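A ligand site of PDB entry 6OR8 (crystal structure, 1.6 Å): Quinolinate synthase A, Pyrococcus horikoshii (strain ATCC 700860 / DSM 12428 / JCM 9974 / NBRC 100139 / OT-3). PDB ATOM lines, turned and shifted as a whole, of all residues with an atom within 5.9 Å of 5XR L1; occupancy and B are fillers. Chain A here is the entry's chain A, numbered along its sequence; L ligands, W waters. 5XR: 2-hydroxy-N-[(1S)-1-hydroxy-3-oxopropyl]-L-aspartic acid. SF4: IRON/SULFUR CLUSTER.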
ATOM      1  N   HIS A  21      14.384  14.607 -12.492  1.00  0.00           N
ATOM      2  CA  HIS A  21      13.326  14.810 -11.524  1.00  0.00           C
ATOM      3  C   HIS A  21      13.412  13.754 -10.410  1.00  0.00           C
ATOM      4  O   HIS A  21      13.988  12.671 -10.583  1.00  0.00           O
ATOM      5  CB  HIS A  21      11.951  14.745 -12.212  1.00  0.00           C
ATOM      6  CG  HIS A  21      10.819  15.113 -11.308  1.00  0.00           C
ATOM      7  ND1 HIS A  21      10.110  14.185 -10.568  1.00  0.00           N
ATOM      8  CD2 HIS A  21      10.299  16.321 -10.995  1.00  0.00           C
ATOM      9  CE1 HIS A  21       9.203  14.811  -9.841  1.00  0.00           C
ATOM     10  NE2 HIS A  21       9.302  16.110 -10.080  1.00  0.00           N
ATOM     11  N   ASN A  22      12.836  14.108  -9.261  1.00  0.00           N
ATOM     12  CA  ASN A  22      12.793  13.239  -8.098  1.00  0.00           C
ATOM     13  C   ASN A  22      12.105  11.894  -8.360  1.00  0.00           C
ATOM     14  O   ASN A  22      12.329  10.945  -7.593  1.00  0.00           O
ATOM     15  CB  ASN A  22      12.055  13.940  -6.935  1.00  0.00           C
ATOM     16  CG  ASN A  22      12.875  15.050  -6.270  1.00  0.00           C
ATOM     17  OD1 ASN A  22      14.091  14.922  -6.083  1.00  0.00           O
ATOM     18  ND2 ASN A  22      12.198  16.128  -5.845  1.00  0.00           N
ATOM     19  N   TYR A  23      11.233  11.783  -9.370  1.00  0.00           N
ATOM     20  CA  TYR A  23      10.589  10.517  -9.698  1.00  0.00           C
ATOM     21  C   TYR A  23      11.379   9.670 -10.670  1.00  0.00           C
ATOM     22  O   TYR A  23      10.870   8.645 -11.131  1.00  0.00           O
ATOM     23  CB  TYR A  23       9.201  10.735 -10.307  1.00  0.00           C
ATOM     24  CG  TYR A  23       8.212  11.463  -9.459  1.00  0.00           C
ATOM     25  CD1 TYR A  23       8.380  11.591  -8.070  1.00  0.00           C
ATOM     26  CD2 TYR A  23       7.099  12.040 -10.047  1.00  0.00           C
ATOM     27  CE1 TYR A  23       7.427  12.270  -7.305  1.00  0.00           C
ATOM     28  CE2 TYR A  23       6.156  12.709  -9.301  1.00  0.00           C
ATOM     29  CZ  TYR A  23       6.324  12.830  -7.939  1.00  0.00           C
ATOM     30  OH  TYR A  23       5.372  13.518  -7.236  1.00  0.00           O
ATOM     31  N   GLY A  36      15.825  17.170  -8.474  1.00  0.00           N
ATOM     32  CA  GLY A  36      14.859  17.935  -7.717  1.00  0.00           C
ATOM     33  C   GLY A  36      13.531  18.019  -8.431  1.00  0.00           C
ATOM     34  O   GLY A  36      13.250  17.225  -9.325  1.00  0.00           O
ATOM     35  N   ASP A  37      12.714  18.991  -8.018  1.00  0.00           N
ATOM     36  CA  ASP A  37      11.498  19.231  -8.784  1.00  0.00           C
ATOM     37  C   ASP A  37      11.818  20.086 -10.015  1.00  0.00           C
ATOM     38  O   ASP A  37      12.944  20.539 -10.215  1.00  0.00           O
ATOM     39  CB  ASP A  37      10.395  19.835  -7.893  1.00  0.00           C
ATOM     40  CG  ASP A  37      10.709  21.225  -7.364  1.00  0.00           C
ATOM     41  OD1 ASP A  37      11.418  22.007  -8.029  1.00  0.00           O
ATOM     42  OD2 ASP A  37      10.173  21.572  -6.286  1.00  0.00           O
ATOM     43  N   SER A  38      10.811  20.264 -10.887  1.00  0.00           N
ATOM     44  CA  SER A  38      11.079  20.819 -12.213  1.00  0.00           C
ATOM     45  C   SER A  38      11.548  22.263 -12.140  1.00  0.00           C
ATOM     46  O   SER A  38      12.466  22.650 -12.881  1.00  0.00           O
ATOM     47  CB  SER A  38       9.845  20.708 -13.119  1.00  0.00           C
ATOM     48  OG  SER A  38       8.742  21.386 -12.584  1.00  0.00           O
ATOM     49  N   LEU A  39      10.929  23.074 -11.273  1.00  0.00           N
ATOM     50  CA  LEU A  39      11.366  24.452 -11.160  1.00  0.00           C
ATOM     51  C   LEU A  39      12.781  24.548 -10.576  1.00  0.00           C
ATOM     52  O   LEU A  39      13.599  25.329 -11.068  1.00  0.00           O
ATOM     53  CB  LEU A  39      10.376  25.261 -10.312  1.00  0.00           C
ATOM     54  CG  LEU A  39      10.721  26.749 -10.160  1.00  0.00           C
ATOM     55  CD1 LEU A  39      10.480  27.523 -11.444  1.00  0.00           C
ATOM     56  CD2 LEU A  39       9.994  27.402  -8.984  1.00  0.00           C
ATOM     57  N   PHE A  60       6.540  19.013 -19.971  1.00  0.00           N
ATOM     58  CA  PHE A  60       6.399  20.391 -19.500  1.00  0.00           C
ATOM     59  C   PHE A  60       7.603  20.836 -18.697  1.00  0.00           C
ATOM     60  O   PHE A  60       7.886  22.035 -18.621  1.00  0.00           O
ATOM     61  CB  PHE A  60       5.112  20.574 -18.661  1.00  0.00           C
ATOM     62  CG  PHE A  60       5.191  20.052 -17.228  1.00  0.00           C
ATOM     63  CD1 PHE A  60       5.834  20.773 -16.221  1.00  0.00           C
ATOM     64  CD2 PHE A  60       4.575  18.866 -16.883  1.00  0.00           C
ATOM     65  CE1 PHE A  60       5.912  20.288 -14.923  1.00  0.00           C
ATOM     66  CE2 PHE A  60       4.629  18.378 -15.590  1.00  0.00           C
ATOM     67  CZ  PHE A  60       5.294  19.081 -14.608  1.00  0.00           C
ATOM     68  N   MET A  61       8.311  19.889 -18.067  1.00  0.00           N
ATOM     69  CA  MET A  61       9.461  20.267 -17.267  1.00  0.00           C
ATOM     70  C   MET A  61      10.624  20.691 -18.170  1.00  0.00           C
ATOM     71  O   MET A  61      11.335  21.648 -17.871  1.00  0.00           O
ATOM     72  CB  MET A  61       9.881  19.111 -16.361  1.00  0.00           C
ATOM     73  CG  MET A  61       8.751  18.463 -15.626  1.00  0.00           C
ATOM     74  SD  MET A  61       9.372  17.160 -14.541  1.00  0.00           S
ATOM     75  CE  MET A  61       7.965  16.884 -13.481  1.00  0.00           C
ATOM     76  N   TYR A 109      -0.422  26.430 -11.952  1.00  0.00           N
ATOM     77  CA  TYR A 109       0.542  25.534 -11.320  1.00  0.00           C
ATOM     78  C   TYR A 109       1.742  25.353 -12.238  1.00  0.00           C
ATOM     79  O   TYR A 109       1.585  25.228 -13.453  1.00  0.00           O
ATOM     80  CB  TYR A 109      -0.165  24.208 -11.044  1.00  0.00           C
ATOM     81  CG  TYR A 109       0.520  23.190 -10.139  1.00  0.00           C
ATOM     82  CD1 TYR A 109       1.483  23.568  -9.202  1.00  0.00           C
ATOM     83  CD2 TYR A 109       0.185  21.843 -10.218  1.00  0.00           C
ATOM     84  CE1 TYR A 109       2.095  22.607  -8.368  1.00  0.00           C
ATOM     85  CE2 TYR A 109       0.775  20.889  -9.400  1.00  0.00           C
ATOM     86  CZ  TYR A 109       1.732  21.272  -8.479  1.00  0.00           C
ATOM     87  OH  TYR A 109       2.297  20.301  -7.671  1.00  0.00           O
ATOM     88  N   VAL A 110       2.956  25.325 -11.653  1.00  0.00           N
ATOM     89  CA  VAL A 110       4.157  25.115 -12.461  1.00  0.00           C
ATOM     90  C   VAL A 110       4.107  23.820 -13.242  1.00  0.00           C
ATOM     91  O   VAL A 110       4.795  23.678 -14.268  1.00  0.00           O
ATOM     92  CB  VAL A 110       5.439  25.185 -11.589  1.00  0.00           C
ATOM     93  CG1 VAL A 110       5.808  26.633 -11.325  1.00  0.00           C
ATOM     94  CG2 VAL A 110       5.246  24.433 -10.279  1.00  0.00           C
ATOM     95  N   ASN A 111       3.328  22.830 -12.784  1.00  0.00           N
ATOM     96  CA  ASN A 111       3.060  21.617 -13.552  1.00  0.00           C
ATOM     97  C   ASN A 111       1.991  21.951 -14.595  1.00  0.00           C
ATOM     98  O   ASN A 111       0.785  21.746 -14.401  1.00  0.00           O
ATOM     99  CB  ASN A 111       2.586  20.472 -12.657  1.00  0.00           C
ATOM    100  CG  ASN A 111       3.544  20.144 -11.532  1.00  0.00           C
ATOM    101  OD1 ASN A 111       4.398  20.939 -11.165  1.00  0.00           O
ATOM    102  ND2 ASN A 111       3.384  18.941 -10.966  1.00  0.00           N
ATOM    103  N   THR A 125       4.061  27.346  -7.176  1.00  0.00           N
ATOM    104  CA  THR A 125       4.511  26.035  -6.720  1.00  0.00           C
ATOM    105  C   THR A 125       3.561  25.542  -5.629  1.00  0.00           C
ATOM    106  O   THR A 125       2.746  26.295  -5.114  1.00  0.00           O
ATOM    107  CB  THR A 125       5.930  26.115  -6.162  1.00  0.00           C
ATOM    108  OG1 THR A 125       5.893  26.901  -4.965  1.00  0.00           O
ATOM    109  CG2 THR A 125       6.882  26.773  -7.159  1.00  0.00           C
ATOM    110  N   SER A 126       3.714  24.273  -5.228  1.00  0.00           N
ATOM    111  CA  SER A 126       2.904  23.795  -4.115  1.00  0.00           C
ATOM    112  C   SER A 126       3.215  24.572  -2.844  1.00  0.00           C
ATOM    113  O   SER A 126       2.314  24.909  -2.062  1.00  0.00           O
ATOM    114  CB  SER A 126       3.142  22.296  -3.882  1.00  0.00           C
ATOM    115  OG  SER A 126       2.881  21.546  -5.060  1.00  0.00           O
ATOM    116  N   CYS A 170      -4.252  14.517 -11.648  1.00  0.00           N
ATOM    117  CA  CYS A 170      -3.138  13.605 -11.923  1.00  0.00           C
ATOM    118  C   CYS A 170      -3.569  12.211 -11.512  1.00  0.00           C
ATOM    119  O   CYS A 170      -3.855  11.984 -10.332  1.00  0.00           O
ATOM    120  CB  CYS A 170      -1.901  14.029 -11.137  1.00  0.00           C
ATOM    121  SG  CYS A 170      -0.673  12.730 -11.012  1.00  0.00           S
ATOM    122  N   HIS A 173      -1.715  10.541  -8.434  1.00  0.00           N
ATOM    123  CA  HIS A 173      -2.063  10.923  -7.078  1.00  0.00           C
ATOM    124  C   HIS A 173      -3.521  10.710  -6.773  1.00  0.00           C
ATOM    125  O   HIS A 173      -3.881  10.542  -5.614  1.00  0.00           O
ATOM    126  CB  HIS A 173      -1.680  12.391  -6.812  1.00  0.00           C
ATOM    127  CG  HIS A 173      -0.201  12.600  -6.809  1.00  0.00           C
ATOM    128  ND1 HIS A 173       0.503  12.880  -7.963  1.00  0.00           N
ATOM    129  CD2 HIS A 173       0.723  12.511  -5.820  1.00  0.00           C
ATOM    130  CE1 HIS A 173       1.787  12.981  -7.670  1.00  0.00           C
ATOM    131  NE2 HIS A 173       1.949  12.766  -6.372  1.00  0.00           N
ATOM    132  N   HIS A 196       1.040  14.670  -1.045  1.00  0.00           N
ATOM    133  CA  HIS A 196       1.112  15.643  -2.141  1.00  0.00           C
ATOM    134  C   HIS A 196      -0.245  16.342  -2.308  1.00  0.00           C
ATOM    135  O   HIS A 196      -1.287  15.707  -2.179  1.00  0.00           O
ATOM    136  CB  HIS A 196       1.488  14.916  -3.435  1.00  0.00           C
ATOM    137  CG  HIS A 196       2.009  15.804  -4.519  1.00  0.00           C
ATOM    138  ND1 HIS A 196       1.224  16.737  -5.172  1.00  0.00           N
ATOM    139  CD2 HIS A 196       3.233  15.889  -5.091  1.00  0.00           C
ATOM    140  CE1 HIS A 196       1.951  17.361  -6.081  1.00  0.00           C
ATOM    141  NE2 HIS A 196       3.177  16.871  -6.054  1.00  0.00           N
ATOM    142  N   GLU A 198      -1.768  17.073  -4.866  1.00  0.00           N
ATOM    143  CA  GLU A 198      -2.561  16.549  -5.966  1.00  0.00           C
ATOM    144  C   GLU A 198      -3.427  15.362  -5.533  1.00  0.00           C
ATOM    145  O   GLU A 198      -4.182  14.838  -6.348  1.00  0.00           O
ATOM    146  CB  GLU A 198      -1.647  16.149  -7.119  1.00  0.00           C
ATOM    147  CG  GLU A 198      -1.050  17.347  -7.885  1.00  0.00           C
ATOM    148  CD  GLU A 198       0.071  16.939  -8.828  1.00  0.00           C
ATOM    149  OE1 GLU A 198       0.305  15.726  -8.994  1.00  0.00           O
ATOM    150  OE2 GLU A 198       0.732  17.816  -9.386  1.00  0.00           O
ATOM    151  N   SER A 212       4.564  19.183  -1.932  1.00  0.00           N
ATOM    152  CA  SER A 212       5.056  18.512  -3.127  1.00  0.00           C
ATOM    153  C   SER A 212       6.471  18.007  -2.830  1.00  0.00           C
ATOM    154  O   SER A 212       6.907  18.027  -1.674  1.00  0.00           O
ATOM    155  CB  SER A 212       5.025  19.446  -4.334  1.00  0.00           C
ATOM    156  OG  SER A 212       5.849  20.561  -4.073  1.00  0.00           O
ATOM    157  N   THR A 213       7.182  17.527  -3.847  1.00  0.00           N
ATOM    158  CA  THR A 213       8.425  16.801  -3.530  1.00  0.00           C
ATOM    159  C   THR A 213       9.472  17.717  -2.929  1.00  0.00           C
ATOM    160  O   THR A 213      10.195  17.307  -2.025  1.00  0.00           O
ATOM    161  CB  THR A 213       8.974  16.073  -4.755  1.00  0.00           C
ATOM    162  OG1 THR A 213       9.452  16.990  -5.765  1.00  0.00           O
ATOM    163  CG2 THR A 213       7.907  15.139  -5.336  1.00  0.00           C
ATOM    164  N   GLY A 214       9.567  18.968  -3.396  1.00  0.00           N
ATOM    165  CA  GLY A 214      10.565  19.864  -2.810  1.00  0.00           C
ATOM    166  C   GLY A 214      10.318  20.121  -1.336  1.00  0.00           C
ATOM    167  O   GLY A 214      11.253  20.110  -0.529  1.00  0.00           O
ATOM    168  N   THR A 230       3.047   9.969  -2.639  1.00  0.00           N
ATOM    169  CA  THR A 230       3.359  10.500  -3.974  1.00  0.00           C
ATOM    170  C   THR A 230       3.932   9.361  -4.782  1.00  0.00           C
ATOM    171  O   THR A 230       3.912   8.201  -4.356  1.00  0.00           O
ATOM    172  CB  THR A 230       4.258  11.752  -3.897  1.00  0.00           C
ATOM    173  OG1 THR A 230       4.282  12.405  -5.177  1.00  0.00           O
ATOM    174  CG2 THR A 230       5.670  11.421  -3.508  1.00  0.00           C
ATOM    175  N   MET A 259       7.266   9.500 -16.570  1.00  0.00           N
ATOM    176  CA  MET A 259       8.614   9.474 -15.996  1.00  0.00           C
ATOM    177  C   MET A 259       9.362   8.219 -16.397  1.00  0.00           C
ATOM    178  O   MET A 259      10.588   8.250 -16.582  1.00  0.00           O
ATOM    179  CB  MET A 259       8.547   9.537 -14.481  1.00  0.00           C
ATOM    180  CG  MET A 259       8.087  10.830 -13.965  1.00  0.00           C
ATOM    181  SD  MET A 259       9.365  12.116 -14.178  1.00  0.00           S
ATOM    182  CE  MET A 259       8.527  13.468 -13.471  1.00  0.00           C
HETATM  183  OAI 5XR L   1       3.378  15.564  -9.627  1.00  0.00           O
HETATM  184  CAH 5XR L   1       4.592  15.784  -9.877  1.00  0.00           C
HETATM  185  OAJ 5XR L   1       5.053  15.726 -11.036  1.00  0.00           O
HETATM  186  CAD 5XR L   1       5.585  16.078  -8.779  1.00  0.00           C
HETATM  187  CAB 5XR L   1       5.951  17.537  -8.745  1.00  0.00           C
HETATM  188  CAA 5XR L   1       6.968  17.648  -7.636  1.00  0.00           C
HETATM  189  OAG 5XR L   1       6.524  18.039  -6.543  1.00  0.00           O
HETATM  190  OAF 5XR L   1       8.160  17.294  -7.827  1.00  0.00           O
HETATM  191  OAC 5XR L   1       4.775  18.228  -8.417  1.00  0.00           O
HETATM  192  NAE 5XR L   1       6.487  18.056  -9.972  1.00  0.00           N
HETATM  193  CAK 5XR L   1       7.469  19.081  -9.721  1.00  0.00           C
HETATM  194  OAO 5XR L   1       8.303  19.229 -10.850  1.00  0.00           O
HETATM  195  CAL 5XR L   1       6.864  20.419  -9.359  1.00  0.00           C
HETATM  196  CAM 5XR L   1       6.230  20.592  -8.007  1.00  0.00           C
HETATM  197  OAN 5XR L   1       5.071  20.908  -8.179  1.00  0.00           O
HETATM  198 FE1  SF4 L   2       3.359  12.340 -13.752  1.00  0.00          FE
HETATM  199 FE2  SF4 L   2       2.179  14.685 -14.443  1.00  0.00          FE
HETATM  200 FE3  SF4 L   2       3.454  14.500 -12.105  1.00  0.00          FE
HETATM  201 FE4  SF4 L   2       1.113  13.241 -12.400  1.00  0.00          FE
HETATM  202  S1  SF4 L   2       1.436  15.395 -12.491  1.00  0.00           S
HETATM  203  S2  SF4 L   2       2.977  12.393 -11.576  1.00  0.00           S
HETATM  204  S3  SF4 L   2       1.285  12.656 -14.539  1.00  0.00           S
HETATM  205  S4  SF4 L   2       4.320  14.277 -14.168  1.00  0.00           S
HETATM  206  O   HOH W   1       8.665  22.529  -9.608  1.00  0.00           O
HETATM  207  O   HOH W   2       7.972  20.327  -5.629  1.00  0.00           O
HETATM  208  O   HOH W   3       5.870  22.928  -6.373  1.00  0.00           O
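The backbone NH (N) of Thr 213 lies within hydrogen-bond range of an oxygen (OAG) of 5XR L1 (2.8 Å).
The side-chain hydroxyl (OG1) of Thr 213 is in hydrogen-bond range of an oxygen (OAF) of 5XR L1.
OAO of 5XR L1 lies within hydrogen-bond range of N of Ser 38 (2.7 Å).
The side-chain hydroxyl (OG) of Ser 38 lies within hydrogen-bond range of an oxygen (OAO) of 5XR L1 (2.8 Å).
A ring nitrogen (NE2) of His 21 sits at hydrogen-bond distance from an oxygen (OAF) of 5XR L1, 2.8 Å away.
An oxygen (OAN) of 5XR L1 lies within hydrogen-bond range of the side-chain hydroxyl (OH) of Tyr 109 (2.9 Å).
OAC of 5XR L1 sits at hydrogen-bond distance from ND2 of Asn 111, at 3.0 Å.
NE2 of His 196 lies within hydrogen-bond range of OAC of 5XR L1, at 3.2 Å.
SG of Cys 170 binds FE4 of SF4 L2.
An oxygen (OAJ) of 5XR L1 binds an iron atom (FE3) of SF4 L2 (2.3 Å).
The backbone NH (N) of Tyr 23 sits at hydrogen-bond distance from a ring nitrogen (ND1) of His 21 (2.9 Å).
OH of Tyr 109 lies close to OE2 of Glu 198.
OG of Ser 126 lies within hydrogen-bond range of OH of Tyr 109, 3.0 Å away.
The side-chain hydroxyl (OG1) of Thr 230 is in hydrogen-bond range of the side-chain hydroxyl (OH) of Tyr 23 (2.6 Å).
The side-chain hydroxyl of Ser 212 sits close to the side-chain hydroxyl of Ser 126, 3.3 Å away.
N of Glu 198 sits at hydrogen-bond distance from ND1 of His 196 (3.0 Å).
N of Leu 39 lies close to OD1 of Asp 37, 3.4 Å away.
ND1 of His 173 lies close to SG of Cys 170 (3.3 Å).
OE1 of Glu 198 sits close to OAI of 5XR L1, at 3.1 Å.
Merely in contact with 5XR L1: Tyr 23, Asp 37, Met 61, Ser 126, His 173 and Ser 212.
Hydrophobic or aromatic side chains that line 5XR L1: His 21, Tyr 23, Met 61, Tyr 109, His 173 and His 196.
Of the 23 residues printed, 13 come within 4 Å of 5XR L1.
The nearest printed residue that does not touch 5XR L1 is Val 110 (4.1 Å).
Water W1 lies within hydrogen-bond range of the backbone NH of Leu 39 (2.9 Å), the side-chain hydroxyl of Ser 38 (3.2 Å) and the side-chain carboxylate of Asp 37 (3.2 Å).
Water W3 lies within hydrogen-bond range of N of Ser 126 (2.8 Å), OAN of 5XR L1 (2.8 Å) and OG of Ser 212 (3.3 Å).
Water W2 lies within hydrogen-bond range of OD2 of Asp 37 (2.6 Å), OG of Ser 212 (2.6 Å), OAG of 5XR L1 (2.9 Å), N of Gly 214 (3.1 Å) and N of Thr 213 (3.4 Å).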
